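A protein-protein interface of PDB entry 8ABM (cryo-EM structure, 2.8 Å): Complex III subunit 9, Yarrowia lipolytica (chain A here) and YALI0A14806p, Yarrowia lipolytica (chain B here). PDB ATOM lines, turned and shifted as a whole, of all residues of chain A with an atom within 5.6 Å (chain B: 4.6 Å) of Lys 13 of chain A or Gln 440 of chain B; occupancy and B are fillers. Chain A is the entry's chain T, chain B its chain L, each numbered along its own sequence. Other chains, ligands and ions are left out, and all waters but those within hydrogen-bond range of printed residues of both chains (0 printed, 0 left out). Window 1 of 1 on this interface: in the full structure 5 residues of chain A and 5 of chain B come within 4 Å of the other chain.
Of the 8 printed residues of chain A, 3 touch a printed residue of chain B.
Printed residues of chain A that touch a printed residue of chain B: Lys 13, Arg 14 and Asn 15.
Of the 10 printed residues of chain B, 3 touch a printed residue of chain A.
Among the printed residues, no Asp or Glu carboxylate lies within 4 Å of a Lys or Arg side-chain nitrogen of the other chain.
The backbone carbonyl oxygen (O) of Ser 374 of chain B is in hydrogen-bond range of the side-chain amide nitrogen (NE2) of Gln 440 of chain B, 2.8 Å away.
The backbone carbonyl oxygen (O) of Ala 439 of chain B lies within hydrogen-bond range of the backbone NH (N) of Tyr 444 of chain B (2.9 Å).
The backbone NH (N) of Lys 13 of chain A is in hydrogen-bond range of the backbone carbonyl oxygen (O) of Tyr 8 of chain A.
OD1 of Asn 9 of chain A is in hydrogen-bond range of NZ of Lys 13 of chain A, at 3.3 Å.
The backbone carbonyl oxygen of Asn 9 of chain A is in hydrogen-bond range of the guanidinium group of Arg 14 of chain A (3.3 Å).
Lys 13 of chain A touches Tyr 444 of chain B.
Trp 474 of chain B touches Arg 14 of chain A.
Val 10 of chain A touches none of the printed residues of chain B.
Phe 11 of chain A touches none of the printed residues of chain B.
Of the printed residues of chain B, Arg 14 of chain A touches Trp 474 (3.6 Å).
Of the printed residues of chain B, Asn 15 of chain A touches Trp 474 (3.3 Å).
Printed residues of chain A within 4 Å of Gln 440 of chain B: Lys 13 (3.2 Å).
Of the printed residues of chain A, Tyr 444 of chain B touches Lys 13.
Printed residues of chain A within 4 Å of Trp 474 of chain B: Arg 14 and Asn 15.
The nearest residue of chain B that does not touch Lys 13 of chain A is Trp 474 of chain B (4.1 Å).
The nearest printed residue of chain B that does not touch Asn 15 of chain A is Tyr 444 of chain B (5.4 Å).
The side-chain amide oxygen of Gln 440 of chain B is in hydrogen-bond range of the side-chain amino group of Lys 13 of chain A, at 3.2 Å.
N of Asn 15 of chain A sits close to O of Trp 474 of chain B (3.4 Å).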
ATOM      1  N   TYR A   8       7.265 -11.956 -17.291  1.00  0.00           N
ATOM      2  CA  TYR A   8       8.299 -12.865 -16.830  1.00  0.00           C
ATOM      3  C   TYR A   8       7.758 -13.768 -15.726  1.00  0.00           C
ATOM      4  O   TYR A   8       7.934 -14.988 -15.791  1.00  0.00           O
ATOM      5  CB  TYR A   8       9.561 -12.134 -16.365  1.00  0.00           C
ATOM      6  CG  TYR A   8      10.534 -13.078 -15.714  1.00  0.00           C
ATOM      7  CD1 TYR A   8      11.414 -13.827 -16.484  1.00  0.00           C
ATOM      8  CD2 TYR A   8      10.529 -13.281 -14.340  1.00  0.00           C
ATOM      9  CE1 TYR A   8      12.280 -14.748 -15.910  1.00  0.00           C
ATOM     10  CE2 TYR A   8      11.387 -14.199 -13.749  1.00  0.00           C
ATOM     11  CZ  TYR A   8      12.277 -14.922 -14.533  1.00  0.00           C
ATOM     12  OH  TYR A   8      13.134 -15.816 -13.956  1.00  0.00           O
ATOM     13  N   ASN A   9       7.134 -13.141 -14.715  1.00  0.00           N
ATOM     14  CA  ASN A   9       6.690 -13.827 -13.510  1.00  0.00           C
ATOM     15  C   ASN A   9       5.658 -14.899 -13.814  1.00  0.00           C
ATOM     16  O   ASN A   9       5.677 -15.962 -13.193  1.00  0.00           O
ATOM     17  CB  ASN A   9       6.075 -12.897 -12.472  1.00  0.00           C
ATOM     18  CG  ASN A   9       7.155 -12.180 -11.706  1.00  0.00           C
ATOM     19  OD1 ASN A   9       8.236 -12.725 -11.505  1.00  0.00           O
ATOM     20  ND2 ASN A   9       6.883 -10.948 -11.316  1.00  0.00           N
ATOM     21  N   VAL A  10       4.792 -14.624 -14.790  1.00  0.00           N
ATOM     22  CA  VAL A  10       3.714 -15.533 -15.109  1.00  0.00           C
ATOM     23  C   VAL A  10       4.192 -16.685 -15.988  1.00  0.00           C
ATOM     24  O   VAL A  10       3.916 -17.834 -15.670  1.00  0.00           O
ATOM     25  CB  VAL A  10       2.513 -14.781 -15.694  1.00  0.00           C
ATOM     26  CG1 VAL A  10       1.418 -15.752 -16.082  1.00  0.00           C
ATOM     27  CG2 VAL A  10       1.977 -13.824 -14.650  1.00  0.00           C
ATOM     28  N   PHE A  11       4.929 -16.401 -17.059  1.00  0.00           N
ATOM     29  CA  PHE A  11       5.107 -17.440 -18.059  1.00  0.00           C
ATOM     30  C   PHE A  11       6.509 -18.026 -18.045  1.00  0.00           C
ATOM     31  O   PHE A  11       6.751 -19.047 -18.686  1.00  0.00           O
ATOM     32  CB  PHE A  11       4.790 -16.899 -19.449  1.00  0.00           C
ATOM     33  CG  PHE A  11       3.356 -16.475 -19.588  1.00  0.00           C
ATOM     34  CD1 PHE A  11       2.349 -17.421 -19.714  1.00  0.00           C
ATOM     35  CD2 PHE A  11       3.007 -15.130 -19.565  1.00  0.00           C
ATOM     36  CE1 PHE A  11       1.022 -17.028 -19.833  1.00  0.00           C
ATOM     37  CE2 PHE A  11       1.680 -14.737 -19.673  1.00  0.00           C
ATOM     38  CZ  PHE A  11       0.691 -15.688 -19.812  1.00  0.00           C
ATOM     39  N   VAL A  12       7.446 -17.368 -17.365  1.00  0.00           N
ATOM     40  CA  VAL A  12       8.827 -17.764 -17.565  1.00  0.00           C
ATOM     41  C   VAL A  12       9.458 -18.246 -16.265  1.00  0.00           C
ATOM     42  O   VAL A  12      10.198 -19.221 -16.274  1.00  0.00           O
ATOM     43  CB  VAL A  12       9.639 -16.639 -18.224  1.00  0.00           C
ATOM     44  CG1 VAL A  12      11.078 -17.054 -18.453  1.00  0.00           C
ATOM     45  CG2 VAL A  12       9.001 -16.274 -19.545  1.00  0.00           C
ATOM     46  N   LYS A  13       9.152 -17.575 -15.154  1.00  0.00           N
ATOM     47  CA  LYS A  13       9.828 -17.822 -13.887  1.00  0.00           C
ATOM     48  C   LYS A  13       9.782 -19.299 -13.488  1.00  0.00           C
ATOM     49  O   LYS A  13      10.826 -19.868 -13.198  1.00  0.00           O
ATOM     50  CB  LYS A  13       9.262 -16.907 -12.800  1.00  0.00           C
ATOM     51  CG  LYS A  13       9.769 -17.148 -11.385  1.00  0.00           C
ATOM     52  CD  LYS A  13       9.394 -16.009 -10.435  1.00  0.00           C
ATOM     53  CE  LYS A  13       7.987 -16.090  -9.880  1.00  0.00           C
ATOM     54  NZ  LYS A  13       7.591 -14.867  -9.137  1.00  0.00           N
ATOM     55  N   ARG A  14       8.586 -19.897 -13.443  1.00  0.00           N
ATOM     56  CA  ARG A  14       8.464 -21.308 -13.134  1.00  0.00           C
ATOM     57  C   ARG A  14       8.685 -22.110 -14.408  1.00  0.00           C
ATOM     58  O   ARG A  14       8.082 -21.809 -15.426  1.00  0.00           O
ATOM     59  CB  ARG A  14       7.068 -21.610 -12.590  1.00  0.00           C
ATOM     60  CG  ARG A  14       6.828 -21.065 -11.195  1.00  0.00           C
ATOM     61  CD  ARG A  14       5.347 -20.865 -10.953  1.00  0.00           C
ATOM     62  NE  ARG A  14       5.137 -20.143  -9.706  1.00  0.00           N
ATOM     63  CZ  ARG A  14       5.054 -18.821  -9.613  1.00  0.00           C
ATOM     64  NH1 ARG A  14       5.132 -18.067 -10.699  1.00  0.00           N
ATOM     65  NH2 ARG A  14       4.874 -18.258  -8.432  1.00  0.00           N
ATOM     66  N   ASN A  15       9.550 -23.122 -14.346  1.00  0.00           N
ATOM     67  CA  ASN A  15       9.818 -23.927 -15.522  1.00  0.00           C
ATOM     68  C   ASN A  15       8.572 -24.692 -15.945  1.00  0.00           C
ATOM     69  O   ASN A  15       8.337 -24.885 -17.131  1.00  0.00           O
ATOM     70  CB  ASN A  15      10.962 -24.916 -15.315  1.00  0.00           C
ATOM     71  CG  ASN A  15      11.529 -25.379 -16.636  1.00  0.00           C
ATOM     72  OD1 ASN A  15      11.740 -24.562 -17.534  1.00  0.00           O
ATOM     73  ND2 ASN A  15      11.804 -26.669 -16.756  1.00  0.00           N
ATOM     74  N   SER B 374      12.850 -19.888  -2.657  1.00  0.00           N
ATOM     75  CA  SER B 374      11.857 -19.473  -3.632  1.00  0.00           C
ATOM     76  C   SER B 374      10.740 -20.496  -3.709  1.00  0.00           C
ATOM     77  O   SER B 374       9.595 -20.107  -3.916  1.00  0.00           O
ATOM     78  CB  SER B 374      12.431 -19.280  -5.000  1.00  0.00           C
ATOM     79  OG  SER B 374      13.244 -18.130  -5.035  1.00  0.00           O
ATOM     80  N   ARG B 436       9.366 -15.956   0.492  1.00  0.00           N
ATOM     81  CA  ARG B 436       9.277 -16.527  -0.846  1.00  0.00           C
ATOM     82  C   ARG B 436       9.232 -15.403  -1.882  1.00  0.00           C
ATOM     83  O   ARG B 436       9.867 -15.509  -2.930  1.00  0.00           O
ATOM     84  CB  ARG B 436       8.046 -17.412  -1.080  1.00  0.00           C
ATOM     85  CG  ARG B 436       8.006 -18.747  -0.349  1.00  0.00           C
ATOM     86  CD  ARG B 436       6.569 -19.229  -0.153  1.00  0.00           C
ATOM     87  NE  ARG B 436       6.151 -19.663  -1.471  1.00  0.00           N
ATOM     88  CZ  ARG B 436       6.623 -20.758  -2.054  1.00  0.00           C
ATOM     89  NH1 ARG B 436       7.488 -21.533  -1.412  1.00  0.00           N
ATOM     90  NH2 ARG B 436       6.227 -21.070  -3.273  1.00  0.00           N
ATOM     91  N   ALA B 437       8.466 -14.337  -1.606  1.00  0.00           N
ATOM     92  CA  ALA B 437       8.341 -13.274  -2.589  1.00  0.00           C
ATOM     93  C   ALA B 437       9.702 -12.641  -2.841  1.00  0.00           C
ATOM     94  O   ALA B 437      10.022 -12.331  -3.984  1.00  0.00           O
ATOM     95  CB  ALA B 437       7.356 -12.228  -2.146  1.00  0.00           C
ATOM     96  N   TRP B 438      10.450 -12.415  -1.755  1.00  0.00           N
ATOM     97  CA  TRP B 438      11.711 -11.713  -1.851  1.00  0.00           C
ATOM     98  C   TRP B 438      12.685 -12.586  -2.616  1.00  0.00           C
ATOM     99  O   TRP B 438      13.390 -12.076  -3.477  1.00  0.00           O
ATOM    100  CB  TRP B 438      12.256 -11.340  -0.477  1.00  0.00           C
ATOM    101  CG  TRP B 438      13.643 -10.784  -0.511  1.00  0.00           C
ATOM    102  CD1 TRP B 438      14.006  -9.482  -0.707  1.00  0.00           C
ATOM    103  CD2 TRP B 438      14.864 -11.523  -0.333  1.00  0.00           C
ATOM    104  NE1 TRP B 438      15.373  -9.366  -0.686  1.00  0.00           N
ATOM    105  CE2 TRP B 438      15.927 -10.596  -0.434  1.00  0.00           C
ATOM    106  CE3 TRP B 438      15.164 -12.872  -0.109  1.00  0.00           C
ATOM    107  CZ2 TRP B 438      17.263 -10.988  -0.338  1.00  0.00           C
ATOM    108  CZ3 TRP B 438      16.486 -13.257   0.002  1.00  0.00           C
ATOM    109  CH2 TRP B 438      17.521 -12.328  -0.115  1.00  0.00           C
ATOM    110  N   ALA B 439      12.701 -13.889  -2.310  1.00  0.00           N
ATOM    111  CA  ALA B 439      13.687 -14.767  -2.918  1.00  0.00           C
ATOM    112  C   ALA B 439      13.427 -14.889  -4.414  1.00  0.00           C
ATOM    113  O   ALA B 439      14.353 -15.008  -5.214  1.00  0.00           O
ATOM    114  CB  ALA B 439      13.658 -16.113  -2.258  1.00  0.00           C
ATOM    115  N   GLN B 440      12.150 -14.847  -4.784  1.00  0.00           N
ATOM    116  CA  GLN B 440      11.794 -15.053  -6.171  1.00  0.00           C
ATOM    117  C   GLN B 440      12.171 -13.829  -6.991  1.00  0.00           C
ATOM    118  O   GLN B 440      12.346 -13.926  -8.199  1.00  0.00           O
ATOM    119  CB  GLN B 440      10.314 -15.353  -6.283  1.00  0.00           C
ATOM    120  CG  GLN B 440      10.025 -16.830  -6.121  1.00  0.00           C
ATOM    121  CD  GLN B 440       8.545 -17.025  -5.927  1.00  0.00           C
ATOM    122  OE1 GLN B 440       7.731 -16.167  -6.257  1.00  0.00           O
ATOM    123  NE2 GLN B 440       8.179 -18.145  -5.337  1.00  0.00           N
ATOM    124  N   LYS B 441      12.315 -12.681  -6.326  1.00  0.00           N
ATOM    125  CA  LYS B 441      12.633 -11.431  -6.996  1.00  0.00           C
ATOM    126  C   LYS B 441      14.142 -11.167  -6.956  1.00  0.00           C
ATOM    127  O   LYS B 441      14.664 -10.461  -7.815  1.00  0.00           O
ATOM    128  CB  LYS B 441      11.671 -10.397  -6.406  1.00  0.00           C
ATOM    129  CG  LYS B 441      12.140  -8.984  -6.118  1.00  0.00           C
ATOM    130  CD  LYS B 441      10.957  -8.133  -5.754  1.00  0.00           C
ATOM    131  CE  LYS B 441      11.187  -7.232  -4.559  1.00  0.00           C
ATOM    132  NZ  LYS B 441      12.289  -6.265  -4.788  1.00  0.00           N
ATOM    133  N   THR B 442      14.848 -11.789  -6.008  1.00  0.00           N
ATOM    134  CA  THR B 442      16.213 -11.399  -5.707  1.00  0.00           C
ATOM    135  C   THR B 442      17.192 -12.530  -5.997  1.00  0.00           C
ATOM    136  O   THR B 442      18.341 -12.276  -6.338  1.00  0.00           O
ATOM    137  CB  THR B 442      16.313 -10.986  -4.237  1.00  0.00           C
ATOM    138  OG1 THR B 442      15.377  -9.929  -4.035  1.00  0.00           O
ATOM    139  CG2 THR B 442      17.699 -10.544  -3.823  1.00  0.00           C
ATOM    140  N   TYR B 444      16.071 -15.996  -7.388  1.00  0.00           N
ATOM    141  CA  TYR B 444      15.708 -17.037  -8.326  1.00  0.00           C
ATOM    142  C   TYR B 444      16.140 -16.641  -9.729  1.00  0.00           C
ATOM    143  O   TYR B 444      15.743 -15.581 -10.208  1.00  0.00           O
ATOM    144  CB  TYR B 444      14.199 -17.256  -8.341  1.00  0.00           C
ATOM    145  CG  TYR B 444      13.907 -18.589  -8.958  1.00  0.00           C
ATOM    146  CD1 TYR B 444      14.229 -19.741  -8.261  1.00  0.00           C
ATOM    147  CD2 TYR B 444      13.426 -18.706 -10.254  1.00  0.00           C
ATOM    148  CE1 TYR B 444      14.028 -21.000  -8.800  1.00  0.00           C
ATOM    149  CE2 TYR B 444      13.224 -19.958 -10.815  1.00  0.00           C
ATOM    150  CZ  TYR B 444      13.533 -21.105 -10.089  1.00  0.00           C
ATOM    151  OH  TYR B 444      13.342 -22.350 -10.618  1.00  0.00           O
ATOM    152  N   TRP B 474      10.763 -27.002 -11.038  1.00  0.00           N
ATOM    153  CA  TRP B 474       9.784 -26.052 -10.556  1.00  0.00           C
ATOM    154  C   TRP B 474       9.368 -25.122 -11.692  1.00  0.00           C
ATOM    155  O   TRP B 474       8.208 -25.253 -12.082  1.00  0.00           O
ATOM    156  CB  TRP B 474      10.381 -25.255  -9.412  1.00  0.00           C
ATOM    157  CG  TRP B 474       9.443 -24.338  -8.698  1.00  0.00           C
ATOM    158  CD1 TRP B 474       8.511 -24.683  -7.765  1.00  0.00           C
ATOM    159  CD2 TRP B 474       9.447 -22.903  -8.749  1.00  0.00           C
ATOM    160  NE1 TRP B 474       7.927 -23.562  -7.245  1.00  0.00           N
ATOM    161  CE2 TRP B 474       8.465 -22.455  -7.839  1.00  0.00           C
ATOM    162  CE3 TRP B 474      10.176 -21.955  -9.471  1.00  0.00           C
ATOM    163  CZ2 TRP B 474       8.199 -21.101  -7.635  1.00  0.00           C
ATOM    164  CZ3 TRP B 474       9.929 -20.612  -9.261  1.00  0.00           C
ATOM    165  CH2 TRP B 474       8.940 -20.192  -8.362  1.00  0.00           C
